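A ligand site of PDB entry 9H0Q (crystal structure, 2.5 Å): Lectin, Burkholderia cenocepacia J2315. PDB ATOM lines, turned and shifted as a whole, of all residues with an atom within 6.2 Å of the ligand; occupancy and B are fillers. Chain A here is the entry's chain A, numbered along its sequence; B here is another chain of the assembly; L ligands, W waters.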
ATOM      1  N   THR A  49     -23.397 -10.681  35.041  1.00  0.00           N
ATOM      2  CA  THR A  49     -23.206 -10.250  33.665  1.00  0.00           C
ATOM      3  C   THR A  49     -24.083  -9.038  33.272  1.00  0.00           C
ATOM      4  O   THR A  49     -24.649  -8.980  32.199  1.00  0.00           O
ATOM      5  CB  THR A  49     -23.426 -11.396  32.684  1.00  0.00           C
ATOM      6  OG1 THR A  49     -23.068 -12.561  33.434  1.00  0.00           O
ATOM      7  CG2 THR A  49     -22.656 -11.111  31.388  1.00  0.00           C
ATOM      8  N   PRO A  50     -24.068  -7.935  34.028  1.00  0.00           N
ATOM      9  CA  PRO A  50     -24.796  -6.733  33.644  1.00  0.00           C
ATOM     10  C   PRO A  50     -24.060  -5.851  32.651  1.00  0.00           C
ATOM     11  O   PRO A  50     -22.850  -5.967  32.516  1.00  0.00           O
ATOM     12  CB  PRO A  50     -24.967  -6.024  35.009  1.00  0.00           C
ATOM     13  CG  PRO A  50     -23.691  -6.368  35.735  1.00  0.00           C
ATOM     14  CD  PRO A  50     -23.240  -7.725  35.219  1.00  0.00           C
ATOM     15  N   TYR A  51     -24.775  -4.886  32.027  1.00  0.00           N
ATOM     16  CA  TYR A  51     -24.114  -3.805  31.319  1.00  0.00           C
ATOM     17  C   TYR A  51     -25.030  -2.593  31.303  1.00  0.00           C
ATOM     18  O   TYR A  51     -26.239  -2.701  31.544  1.00  0.00           O
ATOM     19  CB  TYR A  51     -23.701  -4.196  29.895  1.00  0.00           C
ATOM     20  CG  TYR A  51     -24.786  -4.420  28.860  1.00  0.00           C
ATOM     21  CD1 TYR A  51     -25.444  -5.635  28.744  1.00  0.00           C
ATOM     22  CD2 TYR A  51     -25.121  -3.430  27.958  1.00  0.00           C
ATOM     23  CE1 TYR A  51     -26.425  -5.841  27.785  1.00  0.00           C
ATOM     24  CE2 TYR A  51     -26.044  -3.650  26.956  1.00  0.00           C
ATOM     25  CZ  TYR A  51     -26.729  -4.846  26.875  1.00  0.00           C
ATOM     26  OH  TYR A  51     -27.665  -5.125  25.917  1.00  0.00           O
ATOM     27  N   TYR A  78     -18.366   2.661  33.873  1.00  0.00           N
ATOM     28  CA  TYR A  78     -17.342   2.523  32.860  1.00  0.00           C
ATOM     29  C   TYR A  78     -16.310   3.622  33.040  1.00  0.00           C
ATOM     30  O   TYR A  78     -16.587   4.685  33.660  1.00  0.00           O
ATOM     31  CB  TYR A  78     -17.985   2.561  31.448  1.00  0.00           C
ATOM     32  CG  TYR A  78     -18.881   1.371  31.124  1.00  0.00           C
ATOM     33  CD1 TYR A  78     -18.360   0.104  30.949  1.00  0.00           C
ATOM     34  CD2 TYR A  78     -20.255   1.500  31.093  1.00  0.00           C
ATOM     35  CE1 TYR A  78     -19.160  -0.999  30.703  1.00  0.00           C
ATOM     36  CE2 TYR A  78     -21.067   0.397  30.866  1.00  0.00           C
ATOM     37  CZ  TYR A  78     -20.524  -0.860  30.652  1.00  0.00           C
ATOM     38  OH  TYR A  78     -21.270  -1.944  30.382  1.00  0.00           O
ATOM     39  N   SER A  85     -17.449  -0.366  23.340  1.00  0.00           N
ATOM     40  CA  SER A  85     -18.461  -1.362  23.539  1.00  0.00           C
ATOM     41  C   SER A  85     -18.753  -1.391  25.029  1.00  0.00           C
ATOM     42  O   SER A  85     -17.843  -1.284  25.851  1.00  0.00           O
ATOM     43  CB  SER A  85     -17.984  -2.722  23.043  1.00  0.00           C
ATOM     44  OG  SER A  85     -18.839  -3.773  23.504  1.00  0.00           O
ATOM     45  N   THR A  86     -20.020  -1.558  25.412  1.00  0.00           N
ATOM     46  CA  THR A  86     -20.404  -1.635  26.802  1.00  0.00           C
ATOM     47  C   THR A  86     -20.153  -3.049  27.326  1.00  0.00           C
ATOM     48  O   THR A  86     -20.966  -3.959  27.176  1.00  0.00           O
ATOM     49  CB  THR A  86     -21.860  -1.250  26.941  1.00  0.00           C
ATOM     50  OG1 THR A  86     -22.655  -2.110  26.144  1.00  0.00           O
ATOM     51  CG2 THR A  86     -21.952   0.208  26.550  1.00  0.00           C
ATOM     52  N   GLY A  87     -18.972  -3.207  27.938  1.00  0.00           N
ATOM     53  CA  GLY A  87     -18.529  -4.508  28.395  1.00  0.00           C
ATOM     54  C   GLY A  87     -19.330  -5.014  29.592  1.00  0.00           C
ATOM     55  O   GLY A  87     -19.915  -4.222  30.345  1.00  0.00           O
ATOM     56  N   ARG A  88     -19.359  -6.335  29.741  1.00  0.00           N
ATOM     57  CA  ARG A  88     -20.046  -6.949  30.871  1.00  0.00           C
ATOM     58  C   ARG A  88     -19.229  -6.783  32.148  1.00  0.00           C
ATOM     59  O   ARG A  88     -18.055  -7.115  32.176  1.00  0.00           O
ATOM     60  CB  ARG A  88     -20.310  -8.440  30.605  1.00  0.00           C
ATOM     61  CG  ARG A  88     -21.114  -8.714  29.344  1.00  0.00           C
ATOM     62  CD  ARG A  88     -22.403  -7.921  29.343  1.00  0.00           C
ATOM     63  NE  ARG A  88     -23.197  -8.216  28.151  1.00  0.00           N
ATOM     64  CZ  ARG A  88     -24.440  -8.768  28.225  1.00  0.00           C
ATOM     65  NH1 ARG A  88     -25.041  -9.046  29.373  1.00  0.00           N
ATOM     66  NH2 ARG A  88     -25.072  -9.035  27.109  1.00  0.00           N
ATOM     67  N   ASP A 121     -29.679  -9.617  31.033  1.00  0.00           N
ATOM     68  CA  ASP A 121     -30.186 -10.439  29.962  1.00  0.00           C
ATOM     69  C   ASP A 121     -29.655 -11.857  30.097  1.00  0.00           C
ATOM     70  O   ASP A 121     -29.556 -12.583  29.109  1.00  0.00           O
ATOM     71  CB  ASP A 121     -29.815  -9.825  28.630  1.00  0.00           C
ATOM     72  CG  ASP A 121     -28.310  -9.645  28.422  1.00  0.00           C
ATOM     73  OD1 ASP A 121     -27.491 -10.193  29.226  1.00  0.00           O
ATOM     74  OD2 ASP A 121     -27.986  -8.912  27.458  1.00  0.00           O
ATOM     75  N   SER A 122     -29.309 -12.208  31.327  1.00  0.00           N
ATOM     76  CA  SER A 122     -28.666 -13.493  31.651  1.00  0.00           C
ATOM     77  C   SER A 122     -28.950 -13.716  33.131  1.00  0.00           C
ATOM     78  O   SER A 122     -29.625 -12.905  33.744  1.00  0.00           O
ATOM     79  CB  SER A 122     -27.136 -13.511  31.365  1.00  0.00           C
ATOM     80  OG  SER A 122     -26.504 -12.391  32.013  1.00  0.00           O
ATOM     81  N   TYR A 123     -28.394 -14.791  33.685  1.00  0.00           N
ATOM     82  CA  TYR A 123     -28.649 -15.203  35.059  1.00  0.00           C
ATOM     83  C   TYR A 123     -28.299 -14.132  36.062  1.00  0.00           C
ATOM     84  O   TYR A 123     -27.218 -13.551  35.982  1.00  0.00           O
ATOM     85  CB  TYR A 123     -27.764 -16.441  35.288  1.00  0.00           C
ATOM     86  CG  TYR A 123     -27.892 -16.998  36.701  1.00  0.00           C
ATOM     87  CD1 TYR A 123     -28.854 -17.939  37.048  1.00  0.00           C
ATOM     88  CD2 TYR A 123     -27.029 -16.556  37.691  1.00  0.00           C
ATOM     89  CE1 TYR A 123     -28.934 -18.448  38.340  1.00  0.00           C
ATOM     90  CE2 TYR A 123     -27.099 -17.043  38.983  1.00  0.00           C
ATOM     91  CZ  TYR A 123     -28.030 -18.022  39.297  1.00  0.00           C
ATOM     92  OH  TYR A 123     -28.109 -18.439  40.591  1.00  0.00           O
ATOM     93  N   TYR B  21     -17.559 -25.159  27.432  1.00  0.00           N
ATOM     94  CA  TYR B  21     -17.282 -25.135  28.858  1.00  0.00           C
ATOM     95  C   TYR B  21     -16.334 -26.289  29.186  1.00  0.00           C
ATOM     96  O   TYR B  21     -16.569 -27.401  28.762  1.00  0.00           O
ATOM     97  CB  TYR B  21     -18.574 -25.150  29.673  1.00  0.00           C
ATOM     98  CG  TYR B  21     -19.205 -23.788  29.881  1.00  0.00           C
ATOM     99  CD1 TYR B  21     -18.527 -22.778  30.561  1.00  0.00           C
ATOM    100  CD2 TYR B  21     -20.495 -23.512  29.425  1.00  0.00           C
ATOM    101  CE1 TYR B  21     -19.119 -21.540  30.785  1.00  0.00           C
ATOM    102  CE2 TYR B  21     -21.077 -22.257  29.593  1.00  0.00           C
ATOM    103  CZ  TYR B  21     -20.401 -21.278  30.281  1.00  0.00           C
ATOM    104  OH  TYR B  21     -21.084 -20.091  30.369  1.00  0.00           O
ATOM    105  N   PHE B  57     -12.412  -7.785  21.672  1.00  0.00           N
ATOM    106  CA  PHE B  57     -13.202  -7.522  22.862  1.00  0.00           C
ATOM    107  C   PHE B  57     -13.188  -8.760  23.747  1.00  0.00           C
ATOM    108  O   PHE B  57     -14.187  -9.458  23.934  1.00  0.00           O
ATOM    109  CB  PHE B  57     -14.644  -7.163  22.502  1.00  0.00           C
ATOM    110  CG  PHE B  57     -14.797  -5.846  21.752  1.00  0.00           C
ATOM    111  CD1 PHE B  57     -14.844  -4.647  22.466  1.00  0.00           C
ATOM    112  CD2 PHE B  57     -14.865  -5.815  20.368  1.00  0.00           C
ATOM    113  CE1 PHE B  57     -15.005  -3.465  21.809  1.00  0.00           C
ATOM    114  CE2 PHE B  57     -14.996  -4.590  19.673  1.00  0.00           C
ATOM    115  CZ  PHE B  57     -15.133  -3.416  20.409  1.00  0.00           C
ATOM    116  N   PRO B  58     -12.009  -9.098  24.317  1.00  0.00           N
ATOM    117  CA  PRO B  58     -11.861 -10.346  25.055  1.00  0.00           C
ATOM    118  C   PRO B  58     -12.679 -10.448  26.329  1.00  0.00           C
ATOM    119  O   PRO B  58     -13.173  -9.447  26.853  1.00  0.00           O
ATOM    120  CB  PRO B  58     -10.373 -10.395  25.344  1.00  0.00           C
ATOM    121  CG  PRO B  58      -9.785  -9.456  24.391  1.00  0.00           C
ATOM    122  CD  PRO B  58     -10.772  -8.343  24.238  1.00  0.00           C
ATOM    123  N   TYR B  61     -16.361 -16.601  29.871  1.00  0.00           N
ATOM    124  CA  TYR B  61     -17.617 -17.131  30.386  1.00  0.00           C
ATOM    125  C   TYR B  61     -17.294 -18.077  31.546  1.00  0.00           C
ATOM    126  O   TYR B  61     -16.447 -18.919  31.416  1.00  0.00           O
ATOM    127  CB  TYR B  61     -18.412 -17.952  29.367  1.00  0.00           C
ATOM    128  CG  TYR B  61     -19.081 -17.129  28.272  1.00  0.00           C
ATOM    129  CD1 TYR B  61     -20.207 -16.370  28.526  1.00  0.00           C
ATOM    130  CD2 TYR B  61     -18.597 -17.157  26.965  1.00  0.00           C
ATOM    131  CE1 TYR B  61     -20.832 -15.641  27.521  1.00  0.00           C
ATOM    132  CE2 TYR B  61     -19.200 -16.424  25.957  1.00  0.00           C
ATOM    133  CZ  TYR B  61     -20.334 -15.698  26.211  1.00  0.00           C
ATOM    134  OH  TYR B  61     -20.737 -14.975  25.122  1.00  0.00           O
ATOM    135  N   ASP B  73     -24.470 -19.287  34.819  1.00  0.00           N
ATOM    136  CA  ASP B  73     -23.398 -18.868  33.965  1.00  0.00           C
ATOM    137  C   ASP B  73     -23.367 -17.330  33.921  1.00  0.00           C
ATOM    138  O   ASP B  73     -24.352 -16.621  34.126  1.00  0.00           O
ATOM    139  CB  ASP B  73     -23.458 -19.521  32.582  1.00  0.00           C
ATOM    140  CG  ASP B  73     -24.679 -19.221  31.726  1.00  0.00           C
ATOM    141  OD1 ASP B  73     -25.650 -18.579  32.244  1.00  0.00           O
ATOM    142  OD2 ASP B  73     -24.587 -19.661  30.538  1.00  0.00           O
ATOM    143  N   GLY B  74     -22.198 -16.790  33.574  1.00  0.00           N
ATOM    144  CA  GLY B  74     -22.059 -15.358  33.395  1.00  0.00           C
ATOM    145  C   GLY B  74     -20.750 -15.062  32.687  1.00  0.00           C
ATOM    146  O   GLY B  74     -20.013 -15.964  32.365  1.00  0.00           O
ATOM    147  N   CYS B  75     -20.437 -13.780  32.509  1.00  0.00           N
ATOM    148  CA  CYS B  75     -19.163 -13.427  31.928  1.00  0.00           C
ATOM    149  C   CYS B  75     -18.719 -12.030  32.332  1.00  0.00           C
ATOM    150  O   CYS B  75     -19.525 -11.244  32.745  1.00  0.00           O
ATOM    151  CB  CYS B  75     -19.203 -13.619  30.409  1.00  0.00           C
ATOM    152  SG  CYS B  75     -19.911 -12.235  29.465  1.00  0.00           S
ATOM    153  N   THR B  77     -16.526  -8.978  30.045  1.00  0.00           N
ATOM    154  CA  THR B  77     -15.903  -8.627  28.774  1.00  0.00           C
ATOM    155  C   THR B  77     -15.251  -7.266  28.933  1.00  0.00           C
ATOM    156  O   THR B  77     -15.754  -6.416  29.696  1.00  0.00           O
ATOM    157  CB  THR B  77     -16.924  -8.562  27.638  1.00  0.00           C
ATOM    158  OG1 THR B  77     -17.995  -7.641  27.977  1.00  0.00           O
ATOM    159  CG2 THR B  77     -17.402  -9.976  27.328  1.00  0.00           C
ATOM    160  N   TYR B  78     -14.164  -7.061  28.151  1.00  0.00           N
ATOM    161  CA  TYR B  78     -13.540  -5.747  28.101  1.00  0.00           C
ATOM    162  C   TYR B  78     -14.403  -4.813  27.251  1.00  0.00           C
ATOM    163  O   TYR B  78     -15.185  -5.245  26.412  1.00  0.00           O
ATOM    164  CB  TYR B  78     -12.085  -5.844  27.581  1.00  0.00           C
ATOM    165  CG  TYR B  78     -11.135  -6.613  28.474  1.00  0.00           C
ATOM    166  CD1 TYR B  78     -10.703  -6.060  29.670  1.00  0.00           C
ATOM    167  CD2 TYR B  78     -10.692  -7.879  28.155  1.00  0.00           C
ATOM    168  CE1 TYR B  78      -9.916  -6.789  30.556  1.00  0.00           C
ATOM    169  CE2 TYR B  78      -9.896  -8.608  29.036  1.00  0.00           C
ATOM    170  CZ  TYR B  78      -9.491  -8.048  30.247  1.00  0.00           C
ATOM    171  OH  TYR B  78      -8.677  -8.682  31.120  1.00  0.00           O
ATOM    172  N   VAL B 113     -14.646 -16.195  25.426  1.00  0.00           N
ATOM    173  CA  VAL B 113     -15.381 -15.243  24.615  1.00  0.00           C
ATOM    174  C   VAL B 113     -14.531 -14.882  23.408  1.00  0.00           C
ATOM    175  O   VAL B 113     -13.416 -14.388  23.516  1.00  0.00           O
ATOM    176  CB  VAL B 113     -15.717 -13.966  25.435  1.00  0.00           C
ATOM    177  CG1 VAL B 113     -16.440 -12.917  24.643  1.00  0.00           C
ATOM    178  CG2 VAL B 113     -16.525 -14.284  26.679  1.00  0.00           C
ATOM    179  N   ARG B 114     -15.061 -15.126  22.214  1.00  0.00           N
ATOM    180  CA  ARG B 114     -14.388 -14.710  20.982  1.00  0.00           C
ATOM    181  C   ARG B 114     -12.937 -15.163  20.896  1.00  0.00           C
ATOM    182  O   ARG B 114     -12.053 -14.393  20.538  1.00  0.00           O
ATOM    183  CB  ARG B 114     -14.511 -13.209  20.778  1.00  0.00           C
ATOM    184  CG  ARG B 114     -15.951 -12.744  20.559  1.00  0.00           C
ATOM    185  CD  ARG B 114     -16.059 -11.216  20.386  1.00  0.00           C
ATOM    186  NE  ARG B 114     -16.067 -10.483  21.675  1.00  0.00           N
ATOM    187  CZ  ARG B 114     -17.101 -10.217  22.452  1.00  0.00           C
ATOM    188  NH1 ARG B 114     -16.952  -9.558  23.616  1.00  0.00           N
ATOM    189  NH2 ARG B 114     -18.305 -10.646  22.040  1.00  0.00           N
HETATM  190  C1  LIG L   1     -23.358  -5.752  25.398  1.00  0.00           C
HETATM  191  C2  LIG L   1     -22.441  -6.839  24.831  1.00  0.00           C
HETATM  192  C3  LIG L   1     -21.009  -6.697  25.301  1.00  0.00           C
HETATM  193  C4  LIG L   1     -20.174  -7.829  24.745  1.00  0.00           C
HETATM  194  C5  LIG L   1     -20.825  -9.176  25.031  1.00  0.00           C
HETATM  195  C6  LIG L   1     -22.296  -9.201  24.582  1.00  0.00           C
HETATM  196  O1  LIG L   1     -22.978  -8.112  25.222  1.00  0.00           O
HETATM  197  O2  LIG L   1     -20.055 -10.177  24.379  1.00  0.00           O
HETATM  198  O3  LIG L   1     -18.829  -7.806  25.221  1.00  0.00           O
HETATM  199  O4  LIG L   1     -20.951  -6.570  26.740  1.00  0.00           O
HETATM  200  N1  LIG L   1     -22.992 -10.358  25.008  1.00  0.00           N
HETATM  201  C7  LIG L   1     -23.855 -11.022  24.256  1.00  0.00           C
HETATM  202  O5  LIG L   1     -24.236 -10.535  23.229  1.00  0.00           O
HETATM  203  C8  LIG L   1     -24.317 -12.384  24.634  1.00  0.00           C
HETATM  204  C9  LIG L   1     -25.011 -13.146  23.696  1.00  0.00           C
HETATM  205  C10 LIG L   1     -25.500 -14.393  24.054  1.00  0.00           C
HETATM  206  C11 LIG L   1     -25.288 -14.876  25.345  1.00  0.00           C
HETATM  207  C12 LIG L   1     -24.659 -14.111  26.332  1.00  0.00           C
HETATM  208  C13 LIG L   1     -24.475 -14.610  27.726  1.00  0.00           C
HETATM  209  C14 LIG L   1     -24.397 -15.961  27.984  1.00  0.00           C
HETATM  210  C15 LIG L   1     -24.130 -16.405  29.257  1.00  0.00           C
HETATM  211  C16 LIG L   1     -24.036 -15.534  30.301  1.00  0.00           C
HETATM  212  C17 LIG L   1     -24.095 -14.197  30.070  1.00  0.00           C
HETATM  213  C18 LIG L   1     -24.343 -13.739  28.794  1.00  0.00           C
HETATM  214  C19 LIG L   1     -24.140 -12.874  25.923  1.00  0.00           C
HETATM  215  O   HOH W   1     -17.478  -5.639  24.805  1.00  0.00           O
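The backbone carbonyl oxygen (O) of Thr 86 is in hydrogen-bond range of an oxygen (O4) of the ligand (2.6 Å). OG1 of Thr 77 of chain B lies within hydrogen-bond range of O3 of the ligand, 2.9 Å away. The backbone NH (N) of Arg 88 sits close to an oxygen (O4) of the ligand (3.4 Å). The guanidinium group (NE) of Arg 88 sits at hydrogen-bond distance from an oxygen (O1) of the ligand (2.9 Å). NH2 of Arg 114 of chain B is in hydrogen-bond range of O2 of the ligand.
OG1 of Thr 77 of chain B lies within hydrogen-bond range of N of Arg 88 (2.6 Å). The backbone carbonyl oxygen (O) of Thr 49 lies within hydrogen-bond range of the guanidinium group (NH1) of Arg 88, 2.9 Å away. OD1 of Asp 121 lies within salt-bridge range of NH1 of Arg 88. The backbone carbonyl oxygen (O) of Phe 57 of chain B is in hydrogen-bond range of the guanidinium group (NH1) of Arg 114 of chain B (2.8 Å). OH of Tyr 78 of chain A lies within hydrogen-bond range of O of Gly 87, 2.7 Å away. The side-chain hydroxyl of Thr 49 sits at hydrogen-bond distance from the backbone NH of Cys 75 of chain B, 3.0 Å away.
Thr 49 touches the ligand (CG2 to C17, 3.7 Å). Tyr 51 touches the ligand (CE2 to C1, 3.7 Å). CA of Gly 87 touches O4 of the ligand (3.6 Å). Ser 122 touches the ligand. CE1 of Tyr 61 of chain B touches C14 of the ligand, at 3.6 Å. Asp 73 of chain B touches the ligand. Gly 74 of chain B touches the ligand. Hydrophobic or aromatic side chains that line the ligand: Tyr 51 and Tyr 61 of chain B. Within 4 Å of the ligand: Thr 49, Tyr 51, Thr 86, Gly 87, Arg 88, Ser 122, Tyr 61 of chain B, Asp 73 of chain B, Gly 74 of chain B, Thr 77 of chain B and Arg 114 of chain B. Along chain A the residues within 4 Å of the ligand span positions 49 to 122.
Water W1 lies within hydrogen-bond range of O3 of the ligand, OG of Ser 85 and O of Tyr 78 of chain B.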
